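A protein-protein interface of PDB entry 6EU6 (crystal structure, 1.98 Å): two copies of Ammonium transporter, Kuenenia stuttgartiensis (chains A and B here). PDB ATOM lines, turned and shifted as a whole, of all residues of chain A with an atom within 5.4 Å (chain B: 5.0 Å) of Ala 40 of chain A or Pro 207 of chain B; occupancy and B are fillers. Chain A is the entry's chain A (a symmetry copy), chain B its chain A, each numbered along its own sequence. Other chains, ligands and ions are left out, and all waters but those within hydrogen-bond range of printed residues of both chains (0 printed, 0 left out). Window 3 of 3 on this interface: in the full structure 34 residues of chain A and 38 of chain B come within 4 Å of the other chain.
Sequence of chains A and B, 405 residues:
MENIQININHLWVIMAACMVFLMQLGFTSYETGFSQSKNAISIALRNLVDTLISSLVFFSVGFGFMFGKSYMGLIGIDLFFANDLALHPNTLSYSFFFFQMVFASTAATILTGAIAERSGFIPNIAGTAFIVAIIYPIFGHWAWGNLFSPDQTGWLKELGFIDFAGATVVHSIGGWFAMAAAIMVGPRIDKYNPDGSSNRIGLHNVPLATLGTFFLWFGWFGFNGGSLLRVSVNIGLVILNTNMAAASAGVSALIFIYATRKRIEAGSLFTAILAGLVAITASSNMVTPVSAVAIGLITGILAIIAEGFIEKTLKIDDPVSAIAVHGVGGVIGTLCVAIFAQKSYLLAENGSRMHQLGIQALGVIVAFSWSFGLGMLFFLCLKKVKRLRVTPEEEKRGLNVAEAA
The backbone carbonyl oxygen of Val 206 of chain B is in hydrogen-bond range of the side-chain hydroxyl of Thr 210 of chain B, at 2.8 Å.
The backbone NH of Ile 41 of chain A is in hydrogen-bond range of the side-chain amide oxygen of Asn 400 of chain A, 3.0 Å away.
Among the printed residues, pairs that only touch across the chains: Ala 44 of chain A with Thr 210 of chain B (3.6 Å), Ala 44 of chain A with Pro 207 of chain B (3.8 Å), Ile 41 of chain A with Val 206 of chain B (3.8 Å), Ala 40 of chain A with Pro 207 of chain B (3.9 Å) and Leu 45 of chain A with Val 206 of chain B (3.9 Å).
Printed residues of chain B within 4 Å of Ala 40 of chain A: Pro 207.
Of the printed residues of chain B, Ala 44 of chain A touches Pro 207 (3.8 Å) and Thr 210 (3.6 Å).
Printed residues of chain B within 4 Å of Leu 45 of chain A: Val 206.
The nearest printed residue of chain B that does not touch Ala 40 of chain A is Val 206 of chain B (6.3 Å).
The nearest residue of chain A that does not touch Pro 207 of chain B is Ile 41 of chain A (4.2 Å).
Hydrophobic or aromatic side chains of chain B within 4 Å of the printed part of chain A: Val 206 and Pro 207.
Along chain B the printed residues that touch a printed residue of chain A span positions 206 to 210.
Among the printed residues, 5 pairs touch across the chains.
Among the printed residues, no Asp or Glu carboxylate lies within 4 Å of a Lys or Arg side-chain nitrogen of the other chain.
No position is printed for both chains.
Of the 5 pairs that touch across the chains among the printed residues, none has its exchanged pair printed and touching as well.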
ATOM      1  N   THR A  32      31.042 -28.358 -27.385  1.00  0.00           N
ATOM      2  CA  THR A  32      30.677 -27.002 -27.687  1.00  0.00           C
ATOM      3  C   THR A  32      31.913 -26.103 -27.407  1.00  0.00           C
ATOM      4  O   THR A  32      32.311 -25.297 -28.230  1.00  0.00           O
ATOM      5  CB  THR A  32      29.513 -26.576 -26.871  1.00  0.00           C
ATOM      6  OG1 THR A  32      28.396 -27.404 -27.109  1.00  0.00           O
ATOM      7  CG2 THR A  32      29.108 -25.088 -27.185  1.00  0.00           C
ATOM      8  N   SER A  35      34.446 -26.232 -30.115  1.00  0.00           N
ATOM      9  CA  SER A  35      33.930 -25.882 -31.415  1.00  0.00           C
ATOM     10  C   SER A  35      34.166 -24.383 -31.699  1.00  0.00           C
ATOM     11  O   SER A  35      34.408 -23.566 -30.808  1.00  0.00           O
ATOM     12  CB  SER A  35      32.436 -26.225 -31.506  1.00  0.00           C
ATOM     13  OG  SER A  35      31.549 -25.155 -31.180  1.00  0.00           O
ATOM     14  N   GLN A  36      34.056 -24.053 -32.961  1.00  0.00           N
ATOM     15  CA  GLN A  36      34.032 -22.662 -33.346  1.00  0.00           C
ATOM     16  C   GLN A  36      32.711 -22.153 -32.924  1.00  0.00           C
ATOM     17  O   GLN A  36      31.720 -22.831 -32.988  1.00  0.00           O
ATOM     18  CB  GLN A  36      34.249 -22.512 -34.853  1.00  0.00           C
ATOM     19  CG  GLN A  36      35.650 -23.017 -35.324  1.00  0.00           C
ATOM     20  CD  GLN A  36      35.596 -22.999 -36.849  1.00  0.00           C
ATOM     21  OE1 GLN A  36      35.630 -21.976 -37.449  1.00  0.00           O
ATOM     22  NE2 GLN A  36      35.306 -24.119 -37.424  1.00  0.00           N
ATOM     23  N   SER A  37      32.717 -20.962 -32.406  1.00  0.00           N
ATOM     24  CA  SER A  37      31.528 -20.292 -31.945  1.00  0.00           C
ATOM     25  C   SER A  37      30.334 -20.325 -32.930  1.00  0.00           C
ATOM     26  O   SER A  37      29.199 -20.600 -32.515  1.00  0.00           O
ATOM     27  CB  SER A  37      31.932 -18.872 -31.510  1.00  0.00           C
ATOM     28  OG  SER A  37      30.880 -18.052 -31.798  1.00  0.00           O
ATOM     29  N   LYS A  38      30.562 -20.195 -34.245  1.00  0.00           N
ATOM     30  CA  LYS A  38      29.476 -20.308 -35.240  1.00  0.00           C
ATOM     31  C   LYS A  38      28.758 -21.651 -35.398  1.00  0.00           C
ATOM     32  O   LYS A  38      27.745 -21.769 -36.163  1.00  0.00           O
ATOM     33  CB  LYS A  38      29.995 -19.885 -36.614  1.00  0.00           C
ATOM     34  CG  LYS A  38      31.047 -20.801 -37.164  1.00  0.00           C
ATOM     35  CD  LYS A  38      31.585 -20.276 -38.477  1.00  0.00           C
ATOM     36  CE  LYS A  38      32.614 -21.218 -39.002  1.00  0.00           C
ATOM     37  NZ  LYS A  38      33.116 -20.731 -40.290  1.00  0.00           N
ATOM     38  N   ASN A  39      29.296 -22.681 -34.779  1.00  0.00           N
ATOM     39  CA  ASN A  39      28.721 -24.008 -34.857  1.00  0.00           C
ATOM     40  C   ASN A  39      28.165 -24.557 -33.547  1.00  0.00           C
ATOM     41  O   ASN A  39      27.768 -25.717 -33.504  1.00  0.00           O
ATOM     42  CB  ASN A  39      29.828 -24.973 -35.341  1.00  0.00           C
ATOM     43  CG  ASN A  39      30.223 -24.703 -36.788  1.00  0.00           C
ATOM     44  OD1 ASN A  39      29.386 -24.478 -37.629  1.00  0.00           O
ATOM     45  ND2 ASN A  39      31.521 -24.704 -37.059  1.00  0.00           N
ATOM     46  N   ALA A  40      28.243 -23.757 -32.466  1.00  0.00           N
ATOM     47  CA  ALA A  40      27.903 -24.180 -31.113  1.00  0.00           C
ATOM     48  C   ALA A  40      26.482 -24.680 -31.010  1.00  0.00           C
ATOM     49  O   ALA A  40      26.214 -25.628 -30.296  1.00  0.00           O
ATOM     50  CB  ALA A  40      28.038 -22.999 -30.169  1.00  0.00           C
ATOM     51  N   ILE A  41      25.558 -24.054 -31.753  1.00  0.00           N
ATOM     52  CA  ILE A  41      24.168 -24.507 -31.761  1.00  0.00           C
ATOM     53  C   ILE A  41      24.077 -25.899 -32.316  1.00  0.00           C
ATOM     54  O   ILE A  41      23.349 -26.747 -31.712  1.00  0.00           O
ATOM     55  CB  ILE A  41      23.215 -23.501 -32.518  1.00  0.00           C
ATOM     56  CG1 ILE A  41      23.281 -22.108 -31.833  1.00  0.00           C
ATOM     57  CG2 ILE A  41      21.773 -24.015 -32.517  1.00  0.00           C
ATOM     58  CD1 ILE A  41      22.567 -20.990 -32.626  1.00  0.00           C
ATOM     59  N   SER A  42      24.720 -26.195 -33.459  1.00  0.00           N
ATOM     60  CA  SER A  42      24.492 -27.489 -34.076  1.00  0.00           C
ATOM     61  C   SER A  42      25.048 -28.573 -33.156  1.00  0.00           C
ATOM     62  O   SER A  42      24.515 -29.643 -33.053  1.00  0.00           O
ATOM     63  CB  SER A  42      25.171 -27.694 -35.438  1.00  0.00           C
ATOM     64  OG  SER A  42      26.550 -27.483 -35.322  1.00  0.00           O
ATOM     65  N   ILE A  43      26.193 -28.323 -32.548  1.00  0.00           N
ATOM     66  CA  ILE A  43      26.790 -29.348 -31.761  1.00  0.00           C
ATOM     67  C   ILE A  43      25.984 -29.589 -30.451  1.00  0.00           C
ATOM     68  O   ILE A  43      25.841 -30.735 -30.010  1.00  0.00           O
ATOM     69  CB  ILE A  43      28.334 -29.155 -31.673  1.00  0.00           C
ATOM     70  CG1 ILE A  43      29.009 -30.449 -31.216  1.00  0.00           C
ATOM     71  CG2 ILE A  43      28.687 -27.982 -30.823  1.00  0.00           C
ATOM     72  CD1 ILE A  43      29.025 -31.582 -32.252  1.00  0.00           C
ATOM     73  N   ALA A  44      25.405 -28.550 -29.859  1.00  0.00           N
ATOM     74  CA  ALA A  44      24.579 -28.751 -28.674  1.00  0.00           C
ATOM     75  C   ALA A  44      23.386 -29.637 -29.022  1.00  0.00           C
ATOM     76  O   ALA A  44      23.065 -30.614 -28.325  1.00  0.00           O
ATOM     77  CB  ALA A  44      24.103 -27.419 -28.084  1.00  0.00           C
ATOM     78  N   LEU A  45      22.760 -29.340 -30.137  1.00  0.00           N
ATOM     79  CA  LEU A  45      21.591 -30.076 -30.573  1.00  0.00           C
ATOM     80  C   LEU A  45      21.853 -31.525 -30.976  1.00  0.00           C
ATOM     81  O   LEU A  45      21.017 -32.381 -30.675  1.00  0.00           O
ATOM     82  CB  LEU A  45      20.904 -29.360 -31.716  1.00  0.00           C
ATOM     83  CG  LEU A  45      20.384 -28.008 -31.224  1.00  0.00           C
ATOM     84  CD1 LEU A  45      19.762 -27.303 -32.415  1.00  0.00           C
ATOM     85  CD2 LEU A  45      19.389 -28.103 -30.069  1.00  0.00           C
ATOM     86  N   ASN A 400      24.992 -23.148 -37.527  1.00  0.00           N
ATOM     87  CA  ASN A 400      23.930 -22.440 -36.802  1.00  0.00           C
ATOM     88  C   ASN A 400      23.182 -21.586 -37.818  1.00  0.00           C
ATOM     89  O   ASN A 400      23.400 -20.389 -37.869  1.00  0.00           O
ATOM     90  CB  ASN A 400      24.520 -21.485 -35.755  1.00  0.00           C
ATOM     91  CG  ASN A 400      25.410 -22.178 -34.739  1.00  0.00           C
ATOM     92  OD1 ASN A 400      25.522 -23.389 -34.723  1.00  0.00           O
ATOM     93  ND2 ASN A 400      26.049 -21.391 -33.897  1.00  0.00           N
ATOM     94  N   ASN B 205      20.681 -18.371 -26.519  1.00  0.00           N
ATOM     95  CA  ASN B 205      21.750 -19.233 -26.083  1.00  0.00           C
ATOM     96  C   ASN B 205      21.177 -20.658 -26.023  1.00  0.00           C
ATOM     97  O   ASN B 205      20.864 -21.182 -24.980  1.00  0.00           O
ATOM     98  CB  ASN B 205      22.416 -18.712 -24.827  1.00  0.00           C
ATOM     99  CG  ASN B 205      23.773 -19.375 -24.571  1.00  0.00           C
ATOM    100  OD1 ASN B 205      24.033 -20.488 -24.985  1.00  0.00           O
ATOM    101  ND2 ASN B 205      24.591 -18.728 -23.810  1.00  0.00           N
ATOM    102  N   VAL B 206      21.031 -21.224 -27.212  1.00  0.00           N
ATOM    103  CA  VAL B 206      20.617 -22.564 -27.392  1.00  0.00           C
ATOM    104  C   VAL B 206      21.504 -23.563 -26.666  1.00  0.00           C
ATOM    105  O   VAL B 206      20.972 -24.476 -25.999  1.00  0.00           O
ATOM    106  CB  VAL B 206      20.413 -22.876 -28.860  1.00  0.00           C
ATOM    107  CG1 VAL B 206      20.115 -24.356 -29.099  1.00  0.00           C
ATOM    108  CG2 VAL B 206      19.224 -22.099 -29.331  1.00  0.00           C
ATOM    109  N   PRO B 207      22.839 -23.384 -26.717  1.00  0.00           N
ATOM    110  CA  PRO B 207      23.661 -24.312 -25.921  1.00  0.00           C
ATOM    111  C   PRO B 207      23.320 -24.284 -24.444  1.00  0.00           C
ATOM    112  O   PRO B 207      23.268 -25.322 -23.791  1.00  0.00           O
ATOM    113  CB  PRO B 207      25.105 -23.804 -26.163  1.00  0.00           C
ATOM    114  CG  PRO B 207      25.061 -23.147 -27.500  1.00  0.00           C
ATOM    115  CD  PRO B 207      23.668 -22.580 -27.663  1.00  0.00           C
ATOM    116  N   LEU B 208      23.056 -23.113 -23.893  1.00  0.00           N
ATOM    117  CA  LEU B 208      22.774 -23.027 -22.498  1.00  0.00           C
ATOM    118  C   LEU B 208      21.380 -23.672 -22.168  1.00  0.00           C
ATOM    119  O   LEU B 208      21.245 -24.373 -21.162  1.00  0.00           O
ATOM    120  CB  LEU B 208      22.814 -21.555 -22.068  1.00  0.00           C
ATOM    121  CG  LEU B 208      22.774 -21.299 -20.579  1.00  0.00           C
ATOM    122  CD1 LEU B 208      23.960 -21.907 -19.849  1.00  0.00           C
ATOM    123  CD2 LEU B 208      22.776 -19.795 -20.380  1.00  0.00           C
ATOM    124  N   ALA B 209      20.384 -23.432 -23.013  1.00  0.00           N
ATOM    125  CA  ALA B 209      19.113 -24.139 -22.871  1.00  0.00           C
ATOM    126  C   ALA B 209      19.275 -25.673 -22.966  1.00  0.00           C
ATOM    127  O   ALA B 209      18.556 -26.390 -22.352  1.00  0.00           O
ATOM    128  CB  ALA B 209      18.135 -23.685 -23.916  1.00  0.00           C
ATOM    129  N   THR B 210      20.198 -26.153 -23.779  1.00  0.00           N
ATOM    130  CA  THR B 210      20.467 -27.574 -23.945  1.00  0.00           C
ATOM    131  C   THR B 210      21.046 -28.088 -22.638  1.00  0.00           C
ATOM    132  O   THR B 210      20.606 -29.144 -22.104  1.00  0.00           O
ATOM    133  CB  THR B 210      21.455 -27.819 -25.109  1.00  0.00           C
ATOM    134  OG1 THR B 210      20.907 -27.275 -26.301  1.00  0.00           O
ATOM    135  CG2 THR B 210      21.624 -29.285 -25.365  1.00  0.00           C
ATOM    136  N   LEU B 211      22.001 -27.345 -22.080  1.00  0.00           N
ATOM    137  CA  LEU B 211      22.571 -27.771 -20.807  1.00  0.00           C
ATOM    138  C   LEU B 211      21.441 -27.770 -19.726  1.00  0.00           C
ATOM    139  O   LEU B 211      21.382 -28.695 -18.891  1.00  0.00           O
ATOM    140  CB  LEU B 211      23.764 -26.916 -20.384  1.00  0.00           C
ATOM    141  CG  LEU B 211      24.985 -26.939 -21.324  1.00  0.00           C
ATOM    142  CD1 LEU B 211      26.158 -26.091 -20.789  1.00  0.00           C
ATOM    143  CD2 LEU B 211      25.477 -28.329 -21.639  1.00  0.00           C
